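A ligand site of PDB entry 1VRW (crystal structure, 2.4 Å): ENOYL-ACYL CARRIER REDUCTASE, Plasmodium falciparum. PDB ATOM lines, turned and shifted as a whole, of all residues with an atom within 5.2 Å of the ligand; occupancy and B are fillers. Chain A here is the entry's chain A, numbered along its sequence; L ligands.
The side-chain amino group (NZ) of Lys 189 is in hydrogen-bond range of the backbone carbonyl oxygen (O) of Leu 169 (2.8 Å).
The side-chain hydroxyl (OH) of Tyr 15 sits at hydrogen-bond distance from the backbone carbonyl oxygen (O) of Gly 217, at 2.6 Å.
NE1 of Trp 35 lies within hydrogen-bond range of OD2 of Asp 72.
The side-chain carboxylate (OD1) of Asp 72 lies within hydrogen-bond range of the side-chain hydroxyl (OG) of Ser 74 (2.6 Å).
N of Ala 216 lies within hydrogen-bond range of O of Thr 170 (3.1 Å).
N of Gly 14 is in hydrogen-bond range of OD1 of Asp 11, 3.4 Å away.
The side-chain amino group (NZ) of Lys 189 sits at hydrogen-bond distance from an oxygen (O13) of the ligand (2.7 Å).
N of Tyr 15 sits at hydrogen-bond distance from O8 of the ligand.
The side-chain hydroxyl (OG) of Ser 221 is in hydrogen-bond range of an oxygen (O9) of the ligand (2.8 Å).
N4 of the ligand is in hydrogen-bond range of N of Ala 73 (2.8 Å).
The backbone NH of Ala 223 sits at hydrogen-bond distance from an oxygen (O2) of the ligand (2.9 Å).
N of Leu 219 sits at hydrogen-bond distance from O14 of the ligand (2.9 Å).
A nitrogen (N7) of the ligand sits at hydrogen-bond distance from the backbone carbonyl oxygen (O) of Leu 219 (3.0 Å).
N3 of the ligand is in hydrogen-bond range of OD1 of Asp 72, at 2.9 Å.
N of Gly 10 is in hydrogen-bond range of O5 of the ligand, at 3.2 Å.
The backbone carbonyl oxygen (O) of Leu 120 sits at hydrogen-bond distance from an oxygen (O12) of the ligand (3.3 Å).
N3 of the ligand sits close to NE1 of Trp 35, at 3.5 Å.
Residues that only touch the ligand: Gly 8 (3.9 Å), Ile 9 (3.4 Å), Gly 14 (3.3 Å), Phe 71 (3.5 Å), Ser 74 (3.9 Å), Ser 119 (3.2 Å), Ala 121 (3.5 Å), Asn 122 (3.6 Å), Lys 144 (3.99 Å), Leu 169 (3.4 Å), Thr 170 (3.1 Å), Tyr 171 (3.6 Å), Ala 216 (3.6 Å), Gly 217 (3.6 Å), Pro 218 (3.4 Å), Arg 222 (3.9 Å), Ala 224 (3.5 Å) and Ile 273 (3.5 Å).
Hydrophobic or aromatic side chains that line the ligand: Tyr 15, Trp 35, Ala 73, Leu 120, Ala 121, Leu 169, Tyr 171, Ala 216, Leu 219, Ala 223, Ala 224 and Ile 273.
Of the 35 residues printed, 28 come within 4 Å of the ligand.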
ATOM      1  N   GLY A   8     -25.896  18.289 -10.709  1.00  0.00           N
ATOM      2  CA  GLY A   8     -24.960  19.395 -10.688  1.00  0.00           C
ATOM      3  C   GLY A   8     -23.810  19.264  -9.699  1.00  0.00           C
ATOM      4  O   GLY A   8     -23.730  20.023  -8.736  1.00  0.00           O
ATOM      5  N   ILE A   9     -22.931  18.301  -9.930  1.00  0.00           N
ATOM      6  CA  ILE A   9     -21.767  18.099  -9.089  1.00  0.00           C
ATOM      7  C   ILE A   9     -20.587  17.754  -9.984  1.00  0.00           C
ATOM      8  O   ILE A   9     -20.694  16.902 -10.859  1.00  0.00           O
ATOM      9  CB  ILE A   9     -21.937  16.944  -8.080  1.00  0.00           C
ATOM     10  CG1 ILE A   9     -23.007  17.292  -7.046  1.00  0.00           C
ATOM     11  CG2 ILE A   9     -20.632  16.701  -7.331  1.00  0.00           C
ATOM     12  CD1 ILE A   9     -23.126  16.281  -5.906  1.00  0.00           C
ATOM     13  N   GLY A  10     -19.464  18.428  -9.762  1.00  0.00           N
ATOM     14  CA  GLY A  10     -18.289  18.178 -10.568  1.00  0.00           C
ATOM     15  C   GLY A  10     -17.043  18.129  -9.697  1.00  0.00           C
ATOM     16  O   GLY A  10     -15.930  17.973 -10.191  1.00  0.00           O
ATOM     17  N   ASP A  11     -17.258  18.270  -8.397  1.00  0.00           N
ATOM     18  CA  ASP A  11     -16.164  18.254  -7.433  1.00  0.00           C
ATOM     19  C   ASP A  11     -16.713  18.431  -6.031  1.00  0.00           C
ATOM     20  O   ASP A  11     -17.933  18.470  -5.830  1.00  0.00           O
ATOM     21  CB  ASP A  11     -15.161  19.361  -7.745  1.00  0.00           C
ATOM     22  CG  ASP A  11     -15.823  20.724  -7.830  1.00  0.00           C
ATOM     23  OD1 ASP A  11     -16.382  21.178  -6.810  1.00  0.00           O
ATOM     24  OD2 ASP A  11     -15.778  21.330  -8.919  1.00  0.00           O
ATOM     25  N   ASN A  13     -15.993  21.102  -4.043  1.00  0.00           N
ATOM     26  CA  ASN A  13     -15.933  22.508  -3.644  1.00  0.00           C
ATOM     27  C   ASN A  13     -17.197  23.303  -3.937  1.00  0.00           C
ATOM     28  O   ASN A  13     -17.219  24.522  -3.772  1.00  0.00           O
ATOM     29  CB  ASN A  13     -14.732  23.171  -4.320  1.00  0.00           C
ATOM     30  CG  ASN A  13     -13.446  22.397  -4.104  1.00  0.00           C
ATOM     31  OD1 ASN A  13     -13.110  22.020  -2.983  1.00  0.00           O
ATOM     32  ND2 ASN A  13     -12.717  22.154  -5.197  1.00  0.00           N
ATOM     33  N   GLY A  14     -18.260  22.631  -4.363  1.00  0.00           N
ATOM     34  CA  GLY A  14     -19.482  23.339  -4.657  1.00  0.00           C
ATOM     35  C   GLY A  14     -20.568  23.086  -3.635  1.00  0.00           C
ATOM     36  O   GLY A  14     -20.334  22.414  -2.626  1.00  0.00           O
ATOM     37  N   TYR A  15     -21.758  23.618  -3.896  1.00  0.00           N
ATOM     38  CA  TYR A  15     -22.901  23.447  -3.000  1.00  0.00           C
ATOM     39  C   TYR A  15     -23.479  22.042  -3.056  1.00  0.00           C
ATOM     40  O   TYR A  15     -24.001  21.538  -2.057  1.00  0.00           O
ATOM     41  CB  TYR A  15     -23.986  24.469  -3.337  1.00  0.00           C
ATOM     42  CG  TYR A  15     -23.764  25.824  -2.690  1.00  0.00           C
ATOM     43  CD1 TYR A  15     -23.574  25.939  -1.320  1.00  0.00           C
ATOM     44  CD2 TYR A  15     -23.765  26.997  -3.464  1.00  0.00           C
ATOM     45  CE1 TYR A  15     -23.394  27.183  -0.711  1.00  0.00           C
ATOM     46  CE2 TYR A  15     -23.583  28.249  -2.867  1.00  0.00           C
ATOM     47  CZ  TYR A  15     -23.398  28.327  -1.480  1.00  0.00           C
ATOM     48  OH  TYR A  15     -23.220  29.549  -0.878  1.00  0.00           O
ATOM     49  N   GLY A  16     -23.401  21.413  -4.225  1.00  0.00           N
ATOM     50  CA  GLY A  16     -23.926  20.067  -4.361  1.00  0.00           C
ATOM     51  C   GLY A  16     -23.303  19.141  -3.343  1.00  0.00           C
ATOM     52  O   GLY A  16     -23.978  18.317  -2.729  1.00  0.00           O
ATOM     53  N   TRP A  35     -22.078  16.107 -15.104  1.00  0.00           N
ATOM     54  CA  TRP A  35     -22.019  16.653 -16.446  1.00  0.00           C
ATOM     55  C   TRP A  35     -20.959  15.865 -17.228  1.00  0.00           C
ATOM     56  O   TRP A  35     -19.777  15.893 -16.883  1.00  0.00           O
ATOM     57  CB  TRP A  35     -21.664  18.141 -16.351  1.00  0.00           C
ATOM     58  CG  TRP A  35     -21.796  18.895 -17.626  1.00  0.00           C
ATOM     59  CD1 TRP A  35     -22.770  18.748 -18.578  1.00  0.00           C
ATOM     60  CD2 TRP A  35     -20.947  19.951 -18.091  1.00  0.00           C
ATOM     61  NE1 TRP A  35     -22.585  19.656 -19.589  1.00  0.00           N
ATOM     62  CE2 TRP A  35     -21.472  20.406 -19.317  1.00  0.00           C
ATOM     63  CE3 TRP A  35     -19.797  20.567 -17.577  1.00  0.00           C
ATOM     64  CZ2 TRP A  35     -20.885  21.443 -20.050  1.00  0.00           C
ATOM     65  CZ3 TRP A  35     -19.210  21.605 -18.309  1.00  0.00           C
ATOM     66  CH2 TRP A  35     -19.756  22.028 -19.534  1.00  0.00           C
ATOM     67  N   VAL A  38     -17.037  16.257 -17.483  1.00  0.00           N
ATOM     68  CA  VAL A  38     -16.203  16.082 -16.296  1.00  0.00           C
ATOM     69  C   VAL A  38     -16.441  14.744 -15.610  1.00  0.00           C
ATOM     70  O   VAL A  38     -15.823  14.446 -14.582  1.00  0.00           O
ATOM     71  CB  VAL A  38     -16.431  17.218 -15.273  1.00  0.00           C
ATOM     72  CG1 VAL A  38     -16.403  18.557 -15.982  1.00  0.00           C
ATOM     73  CG2 VAL A  38     -17.743  17.023 -14.538  1.00  0.00           C
ATOM     74  N   PHE A  71     -24.852  12.988 -16.694  1.00  0.00           N
ATOM     75  CA  PHE A  71     -26.117  13.691 -16.809  1.00  0.00           C
ATOM     76  C   PHE A  71     -25.957  15.079 -17.421  1.00  0.00           C
ATOM     77  O   PHE A  71     -25.153  15.879 -16.957  1.00  0.00           O
ATOM     78  CB  PHE A  71     -26.731  13.801 -15.401  1.00  0.00           C
ATOM     79  CG  PHE A  71     -27.923  14.698 -15.322  1.00  0.00           C
ATOM     80  CD1 PHE A  71     -29.187  14.254 -15.703  1.00  0.00           C
ATOM     81  CD2 PHE A  71     -27.787  16.014 -14.870  1.00  0.00           C
ATOM     82  CE1 PHE A  71     -30.302  15.098 -15.622  1.00  0.00           C
ATOM     83  CE2 PHE A  71     -28.890  16.866 -14.790  1.00  0.00           C
ATOM     84  CZ  PHE A  71     -30.143  16.409 -15.161  1.00  0.00           C
ATOM     85  N   ASP A  72     -26.731  15.357 -18.461  1.00  0.00           N
ATOM     86  CA  ASP A  72     -26.671  16.662 -19.111  1.00  0.00           C
ATOM     87  C   ASP A  72     -28.047  17.310 -19.133  1.00  0.00           C
ATOM     88  O   ASP A  72     -28.955  16.856 -19.845  1.00  0.00           O
ATOM     89  CB  ASP A  72     -26.132  16.542 -20.528  1.00  0.00           C
ATOM     90  CG  ASP A  72     -25.646  17.858 -21.062  1.00  0.00           C
ATOM     91  OD1 ASP A  72     -26.358  18.859 -20.848  1.00  0.00           O
ATOM     92  OD2 ASP A  72     -24.572  17.908 -21.681  1.00  0.00           O
ATOM     93  N   ALA A  73     -28.190  18.388 -18.359  1.00  0.00           N
ATOM     94  CA  ALA A  73     -29.445  19.118 -18.231  1.00  0.00           C
ATOM     95  C   ALA A  73     -29.941  19.820 -19.483  1.00  0.00           C
ATOM     96  O   ALA A  73     -31.078  20.287 -19.531  1.00  0.00           O
ATOM     97  CB  ALA A  73     -29.334  20.110 -17.098  1.00  0.00           C
ATOM     98  N   SER A  74     -29.114  19.896 -20.510  1.00  0.00           N
ATOM     99  CA  SER A  74     -29.517  20.574 -21.739  1.00  0.00           C
ATOM    100  C   SER A  74     -30.261  19.660 -22.717  1.00  0.00           C
ATOM    101  O   SER A  74     -30.725  20.130 -23.753  1.00  0.00           O
ATOM    102  CB  SER A  74     -28.300  21.182 -22.424  1.00  0.00           C
ATOM    103  OG  SER A  74     -27.381  20.173 -22.800  1.00  0.00           O
ATOM    104  N   SER A 119     -28.884  21.656  -8.697  1.00  0.00           N
ATOM    105  CA  SER A 119     -27.747  22.445  -8.241  1.00  0.00           C
ATOM    106  C   SER A 119     -26.795  22.749  -9.386  1.00  0.00           C
ATOM    107  O   SER A 119     -25.583  22.575  -9.259  1.00  0.00           O
ATOM    108  CB  SER A 119     -27.012  21.660  -7.145  1.00  0.00           C
ATOM    109  OG  SER A 119     -25.910  22.384  -6.635  1.00  0.00           O
ATOM    110  N   LEU A 120     -27.331  23.219 -10.501  1.00  0.00           N
ATOM    111  CA  LEU A 120     -26.497  23.514 -11.644  1.00  0.00           C
ATOM    112  C   LEU A 120     -26.807  24.841 -12.310  1.00  0.00           C
ATOM    113  O   LEU A 120     -27.947  25.306 -12.317  1.00  0.00           O
ATOM    114  CB  LEU A 120     -26.634  22.386 -12.667  1.00  0.00           C
ATOM    115  CG  LEU A 120     -28.031  22.246 -13.258  1.00  0.00           C
ATOM    116  CD1 LEU A 120     -28.054  22.966 -14.598  1.00  0.00           C
ATOM    117  CD2 LEU A 120     -28.403  20.780 -13.444  1.00  0.00           C
ATOM    118  N   ALA A 121     -25.764  25.456 -12.871  1.00  0.00           N
ATOM    119  CA  ALA A 121     -25.883  26.731 -13.560  1.00  0.00           C
ATOM    120  C   ALA A 121     -24.849  26.774 -14.679  1.00  0.00           C
ATOM    121  O   ALA A 121     -23.791  26.137 -14.586  1.00  0.00           O
ATOM    122  CB  ALA A 121     -25.658  27.881 -12.587  1.00  0.00           C
ATOM    123  N   ASN A 122     -25.150  27.503 -15.738  1.00  0.00           N
ATOM    124  CA  ASN A 122     -24.217  27.617 -16.851  1.00  0.00           C
ATOM    125  C   ASN A 122     -24.649  28.696 -17.823  1.00  0.00           C
ATOM    126  O   ASN A 122     -25.804  28.740 -18.245  1.00  0.00           O
ATOM    127  CB  ASN A 122     -24.090  26.300 -17.600  1.00  0.00           C
ATOM    128  CG  ASN A 122     -22.986  26.342 -18.640  1.00  0.00           C
ATOM    129  OD1 ASN A 122     -21.803  26.334 -18.302  1.00  0.00           O
ATOM    130  ND2 ASN A 122     -23.364  26.398 -19.916  1.00  0.00           N
ATOM    131  N   LYS A 144     -30.049  26.113 -19.873  1.00  0.00           N
ATOM    132  CA  LYS A 144     -29.303  25.321 -18.918  1.00  0.00           C
ATOM    133  C   LYS A 144     -29.589  25.596 -17.444  1.00  0.00           C
ATOM    134  O   LYS A 144     -29.685  24.665 -16.642  1.00  0.00           O
ATOM    135  CB  LYS A 144     -27.797  25.487 -19.152  1.00  0.00           C
ATOM    136  CG  LYS A 144     -27.191  24.621 -20.245  1.00  0.00           C
ATOM    137  CD  LYS A 144     -27.553  25.090 -21.635  1.00  0.00           C
ATOM    138  CE  LYS A 144     -26.646  24.441 -22.682  1.00  0.00           C
ATOM    139  NZ  LYS A 144     -25.220  24.868 -22.546  1.00  0.00           N
ATOM    140  N   LEU A 169     -30.959  26.048  -6.268  1.00  0.00           N
ATOM    141  CA  LEU A 169     -30.164  27.134  -5.698  1.00  0.00           C
ATOM    142  C   LEU A 169     -30.290  28.400  -6.548  1.00  0.00           C
ATOM    143  O   LEU A 169     -30.270  28.344  -7.778  1.00  0.00           O
ATOM    144  CB  LEU A 169     -28.698  26.725  -5.604  1.00  0.00           C
ATOM    145  CG  LEU A 169     -28.221  25.727  -4.536  1.00  0.00           C
ATOM    146  CD1 LEU A 169     -28.542  26.265  -3.157  1.00  0.00           C
ATOM    147  CD2 LEU A 169     -28.897  24.384  -4.719  1.00  0.00           C
ATOM    148  N   THR A 170     -30.431  29.541  -5.895  1.00  0.00           N
ATOM    149  CA  THR A 170     -30.549  30.803  -6.601  1.00  0.00           C
ATOM    150  C   THR A 170     -29.656  31.848  -5.915  1.00  0.00           C
ATOM    151  O   THR A 170     -29.050  31.577  -4.879  1.00  0.00           O
ATOM    152  CB  THR A 170     -32.037  31.257  -6.651  1.00  0.00           C
ATOM    153  OG1 THR A 170     -32.179  32.339  -7.585  1.00  0.00           O
ATOM    154  CG2 THR A 170     -32.500  31.711  -5.281  1.00  0.00           C
ATOM    155  N   TYR A 171     -29.562  33.035  -6.519  1.00  0.00           N
ATOM    156  CA  TYR A 171     -28.722  34.086  -5.966  1.00  0.00           C
ATOM    157  C   TYR A 171     -29.466  35.423  -6.071  1.00  0.00           C
ATOM    158  O   TYR A 171     -30.147  35.690  -7.070  1.00  0.00           O
ATOM    159  CB  TYR A 171     -27.386  34.120  -6.718  1.00  0.00           C
ATOM    160  CG  TYR A 171     -26.381  35.138  -6.214  1.00  0.00           C
ATOM    161  CD1 TYR A 171     -25.983  35.169  -4.869  1.00  0.00           C
ATOM    162  CD2 TYR A 171     -25.828  36.077  -7.078  1.00  0.00           C
ATOM    163  CE1 TYR A 171     -25.059  36.114  -4.409  1.00  0.00           C
ATOM    164  CE2 TYR A 171     -24.902  37.029  -6.630  1.00  0.00           C
ATOM    165  CZ  TYR A 171     -24.535  37.042  -5.293  1.00  0.00           C
ATOM    166  OH  TYR A 171     -23.645  38.004  -4.853  1.00  0.00           O
ATOM    167  N   TYR A 181     -22.300  39.860 -12.327  1.00  0.00           N
ATOM    168  CA  TYR A 181     -23.107  38.666 -12.568  1.00  0.00           C
ATOM    169  C   TYR A 181     -23.820  38.842 -13.907  1.00  0.00           C
ATOM    170  O   TYR A 181     -25.027  39.113 -13.935  1.00  0.00           O
ATOM    171  CB  TYR A 181     -24.133  38.510 -11.446  1.00  0.00           C
ATOM    172  CG  TYR A 181     -24.572  37.109 -11.134  1.00  0.00           C
ATOM    173  CD1 TYR A 181     -23.719  36.214 -10.472  1.00  0.00           C
ATOM    174  CD2 TYR A 181     -25.853  36.667 -11.472  1.00  0.00           C
ATOM    175  CE1 TYR A 181     -24.133  34.930 -10.154  1.00  0.00           C
ATOM    176  CE2 TYR A 181     -26.280  35.389 -11.153  1.00  0.00           C
ATOM    177  CZ  TYR A 181     -25.423  34.524 -10.496  1.00  0.00           C
ATOM    178  OH  TYR A 181     -25.861  33.259 -10.187  1.00  0.00           O
ATOM    179  N   MET A 185     -27.293  35.444 -16.454  1.00  0.00           N
ATOM    180  CA  MET A 185     -27.392  34.646 -15.236  1.00  0.00           C
ATOM    181  C   MET A 185     -28.387  35.250 -14.250  1.00  0.00           C
ATOM    182  O   MET A 185     -29.116  34.524 -13.588  1.00  0.00           O
ATOM    183  CB  MET A 185     -26.019  34.502 -14.573  1.00  0.00           C
ATOM    184  CG  MET A 185     -25.224  33.316 -15.062  1.00  0.00           C
ATOM    185  SD  MET A 185     -26.187  31.793 -14.921  1.00  0.00           S
ATOM    186  CE  MET A 185     -26.334  31.660 -13.159  1.00  0.00           C
ATOM    187  N   LYS A 189     -31.842  33.369 -13.003  1.00  0.00           N
ATOM    188  CA  LYS A 189     -32.215  33.206 -11.605  1.00  0.00           C
ATOM    189  C   LYS A 189     -33.582  33.821 -11.321  1.00  0.00           C
ATOM    190  O   LYS A 189     -34.341  33.313 -10.499  1.00  0.00           O
ATOM    191  CB  LYS A 189     -31.152  33.809 -10.692  1.00  0.00           C
ATOM    192  CG  LYS A 189     -29.817  33.058 -10.720  1.00  0.00           C
ATOM    193  CD  LYS A 189     -29.991  31.590 -10.335  1.00  0.00           C
ATOM    194  CE  LYS A 189     -28.646  30.899 -10.234  1.00  0.00           C
ATOM    195  NZ  LYS A 189     -28.750  29.451  -9.903  1.00  0.00           N
ATOM    196  N   ALA A 216     -28.519  31.335  -1.789  1.00  0.00           N
ATOM    197  CA  ALA A 216     -27.283  31.262  -1.040  1.00  0.00           C
ATOM    198  C   ALA A 216     -26.381  32.476  -1.158  1.00  0.00           C
ATOM    199  O   ALA A 216     -26.520  33.292  -2.064  1.00  0.00           O
ATOM    200  CB  ALA A 216     -26.513  30.012  -1.463  1.00  0.00           C
ATOM    201  N   GLY A 217     -25.451  32.574  -0.219  1.00  0.00           N
ATOM    202  CA  GLY A 217     -24.471  33.644  -0.216  1.00  0.00           C
ATOM    203  C   GLY A 217     -23.289  33.175  -1.056  1.00  0.00           C
ATOM    204  O   GLY A 217     -23.320  32.063  -1.579  1.00  0.00           O
ATOM    205  N   PRO A 218     -22.231  33.983  -1.184  1.00  0.00           N
ATOM    206  CA  PRO A 218     -21.040  33.634  -1.977  1.00  0.00           C
ATOM    207  C   PRO A 218     -20.282  32.413  -1.515  1.00  0.00           C
ATOM    208  O   PRO A 218     -20.104  32.191  -0.314  1.00  0.00           O
ATOM    209  CB  PRO A 218     -20.162  34.894  -1.870  1.00  0.00           C
ATOM    210  CG  PRO A 218     -21.101  35.966  -1.368  1.00  0.00           C
ATOM    211  CD  PRO A 218     -21.994  35.229  -0.437  1.00  0.00           C
ATOM    212  N   LEU A 219     -19.836  31.605  -2.473  1.00  0.00           N
ATOM    213  CA  LEU A 219     -19.060  30.408  -2.199  1.00  0.00           C
ATOM    214  C   LEU A 219     -18.024  30.287  -3.317  1.00  0.00           C
ATOM    215  O   LEU A 219     -18.373  30.271  -4.499  1.00  0.00           O
ATOM    216  CB  LEU A 219     -19.951  29.156  -2.182  1.00  0.00           C
ATOM    217  CG  LEU A 219     -19.247  27.878  -1.716  1.00  0.00           C
ATOM    218  CD1 LEU A 219     -19.017  27.958  -0.217  1.00  0.00           C
ATOM    219  CD2 LEU A 219     -20.087  26.647  -2.047  1.00  0.00           C
ATOM    220  N   LYS A 220     -16.752  30.204  -2.938  1.00  0.00           N
ATOM    221  CA  LYS A 220     -15.685  30.096  -3.914  1.00  0.00           C
ATOM    222  C   LYS A 220     -15.640  28.682  -4.500  1.00  0.00           C
ATOM    223  O   LYS A 220     -14.884  27.818  -4.047  1.00  0.00           O
ATOM    224  CB  LYS A 220     -14.338  30.442  -3.278  1.00  0.00           C
ATOM    225  CG  LYS A 220     -13.223  30.670  -4.286  1.00  0.00           C
ATOM    226  CD  LYS A 220     -11.974  31.201  -3.617  1.00  0.00           C
ATOM    227  CE  LYS A 220     -10.915  31.580  -4.644  1.00  0.00           C
ATOM    228  NZ  LYS A 220     -11.414  32.620  -5.592  1.00  0.00           N
ATOM    229  N   SER A 221     -16.484  28.456  -5.503  1.00  0.00           N
ATOM    230  CA  SER A 221     -16.554  27.158  -6.166  1.00  0.00           C
ATOM    231  C   SER A 221     -16.105  27.355  -7.623  1.00  0.00           C
ATOM    232  O   SER A 221     -15.780  28.466  -8.028  1.00  0.00           O
ATOM    233  CB  SER A 221     -17.983  26.639  -6.140  1.00  0.00           C
ATOM    234  OG  SER A 221     -18.853  27.518  -6.824  1.00  0.00           O
ATOM    235  N   ARG A 222     -16.101  26.272  -8.387  1.00  0.00           N
ATOM    236  CA  ARG A 222     -15.681  26.341  -9.781  1.00  0.00           C
ATOM    237  C   ARG A 222     -16.567  27.294 -10.589  1.00  0.00           C
ATOM    238  O   ARG A 222     -16.063  28.217 -11.239  1.00  0.00           O
ATOM    239  CB  ARG A 222     -15.710  24.948 -10.415  1.00  0.00           C
ATOM    240  CG  ARG A 222     -14.817  24.825 -11.634  1.00  0.00           C
ATOM    241  CD  ARG A 222     -14.947  23.454 -12.285  1.00  0.00           C
ATOM    242  NE  ARG A 222     -13.919  23.242 -13.294  1.00  0.00           N
ATOM    243  CZ  ARG A 222     -13.681  24.058 -14.324  1.00  0.00           C
ATOM    244  NH1 ARG A 222     -14.402  25.165 -14.479  1.00  0.00           N
ATOM    245  NH2 ARG A 222     -12.719  23.775 -15.194  1.00  0.00           N
ATOM    246  N   ALA A 223     -17.881  27.077 -10.558  1.00  0.00           N
ATOM    247  CA  ALA A 223     -18.810  27.921 -11.300  1.00  0.00           C
ATOM    248  C   ALA A 223     -18.627  29.404 -10.959  1.00  0.00           C
ATOM    249  O   ALA A 223     -18.612  30.255 -11.853  1.00  0.00           O
ATOM    250  CB  ALA A 223     -20.252  27.497 -10.998  1.00  0.00           C
ATOM    251  N   ALA A 224     -18.471  29.703  -9.668  1.00  0.00           N
ATOM    252  CA  ALA A 224     -18.291  31.067  -9.202  1.00  0.00           C
ATOM    253  C   ALA A 224     -16.968  31.667  -9.678  1.00  0.00           C
ATOM    254  O   ALA A 224     -16.943  32.764 -10.242  1.00  0.00           O
ATOM    255  CB  ALA A 224     -18.350  31.106  -7.672  1.00  0.00           C
ATOM    256  N   ILE A 273     -16.166  36.646  -7.412  1.00  0.00           N
ATOM    257  CA  ILE A 273     -16.418  35.857  -6.211  1.00  0.00           C
ATOM    258  C   ILE A 273     -15.595  36.272  -4.997  1.00  0.00           C
ATOM    259  O   ILE A 273     -16.077  36.240  -3.863  1.00  0.00           O
ATOM    260  CB  ILE A 273     -16.217  34.338  -6.491  1.00  0.00           C
ATOM    261  CG1 ILE A 273     -16.978  33.514  -5.443  1.00  0.00           C
ATOM    262  CG2 ILE A 273     -14.733  33.969  -6.444  1.00  0.00           C
ATOM    263  CD1 ILE A 273     -18.476  33.758  -5.439  1.00  0.00           C
HETATM  264  P1  LIG L   1     -20.441  24.215  -9.027  1.00  0.00           P
HETATM  265  O1  LIG L   1     -19.866  23.192  -8.081  1.00  0.00           O
HETATM  266  O2  LIG L   1     -19.545  24.759 -10.113  1.00  0.00           O
HETATM  267  O3  LIG L   1     -21.769  23.479  -9.657  1.00  0.00           O
HETATM  268  C1  LIG L   1     -22.421  23.710 -10.933  1.00  0.00           C
HETATM  269  C2  LIG L   1     -22.466  22.435 -11.714  1.00  0.00           C
HETATM  270  O4  LIG L   1     -23.297  22.490 -12.921  1.00  0.00           O
HETATM  271  C3  LIG L   1     -21.071  22.002 -12.188  1.00  0.00           C
HETATM  272  O5  LIG L   1     -20.676  20.915 -11.305  1.00  0.00           O
HETATM  273  C4  LIG L   1     -21.240  21.572 -13.655  1.00  0.00           C
HETATM  274  O6  LIG L   1     -20.557  20.376 -13.894  1.00  0.00           O
HETATM  275  C5  LIG L   1     -22.776  21.519 -13.857  1.00  0.00           C
HETATM  276  N1  LIG L   1     -23.234  21.917 -15.232  1.00  0.00           N
HETATM  277  C6  LIG L   1     -23.099  22.895 -16.194  1.00  0.00           C
HETATM  278  N2  LIG L   1     -23.803  22.706 -17.305  1.00  0.00           N
HETATM  279  C7  LIG L   1     -24.466  21.513 -17.068  1.00  0.00           C
HETATM  280  C8  LIG L   1     -25.348  20.751 -17.853  1.00  0.00           C
HETATM  281  N3  LIG L   1     -25.723  21.098 -19.070  1.00  0.00           N
HETATM  282  N4  LIG L   1     -25.834  19.607 -17.332  1.00  0.00           N
HETATM  283  C9  LIG L   1     -25.499  19.261 -16.071  1.00  0.00           C
HETATM  284  N5  LIG L   1     -24.613  19.836 -15.255  1.00  0.00           N
HETATM  285  C10 LIG L   1     -24.132  21.009 -15.792  1.00  0.00           C
HETATM  286  O7  LIG L   1     -20.913  25.566  -8.523  1.00  0.00           O
HETATM  287  P2  LIG L   1     -21.829  26.012  -7.434  1.00  0.00           P
HETATM  288  O8  LIG L   1     -21.764  25.158  -6.195  1.00  0.00           O
HETATM  289  O9  LIG L   1     -21.583  27.469  -7.316  1.00  0.00           O
HETATM  290  O10 LIG L   1     -23.241  26.069  -8.187  1.00  0.00           O
HETATM  291  C11 LIG L   1     -24.373  25.237  -7.889  1.00  0.00           C
HETATM  292  C12 LIG L   1     -25.627  26.141  -7.832  1.00  0.00           C
HETATM  293  O11 LIG L   1     -25.523  27.097  -6.699  1.00  0.00           O
HETATM  294  C13 LIG L   1     -25.765  26.958  -9.116  1.00  0.00           C
HETATM  295  O12 LIG L   1     -27.079  26.802  -9.543  1.00  0.00           O
HETATM  296  C14 LIG L   1     -25.447  28.341  -8.660  1.00  0.00           C
HETATM  297  O13 LIG L   1     -26.088  29.306  -9.448  1.00  0.00           O
HETATM  298  C15 LIG L   1     -25.958  28.344  -7.248  1.00  0.00           C
HETATM  299  N6  LIG L   1     -25.485  29.470  -6.426  1.00  0.00           N
HETATM  300  C16 LIG L   1     -24.072  29.651  -6.277  1.00  0.00           C
HETATM  301  C17 LIG L   1     -23.401  30.667  -5.602  1.00  0.00           C
HETATM  302  C18 LIG L   1     -21.941  30.825  -5.435  1.00  0.00           C
HETATM  303  O14 LIG L   1     -21.364  31.928  -4.939  1.00  0.00           O
HETATM  304  N7  LIG L   1     -21.041  29.896  -5.727  1.00  0.00           N
HETATM  305  C19 LIG L   1     -24.346  31.476  -4.960  1.00  0.00           C
HETATM  306  C20 LIG L   1     -25.777  31.358  -4.965  1.00  0.00           C
HETATM  307  C21 LIG L   1     -26.367  30.294  -5.756  1.00  0.00           C
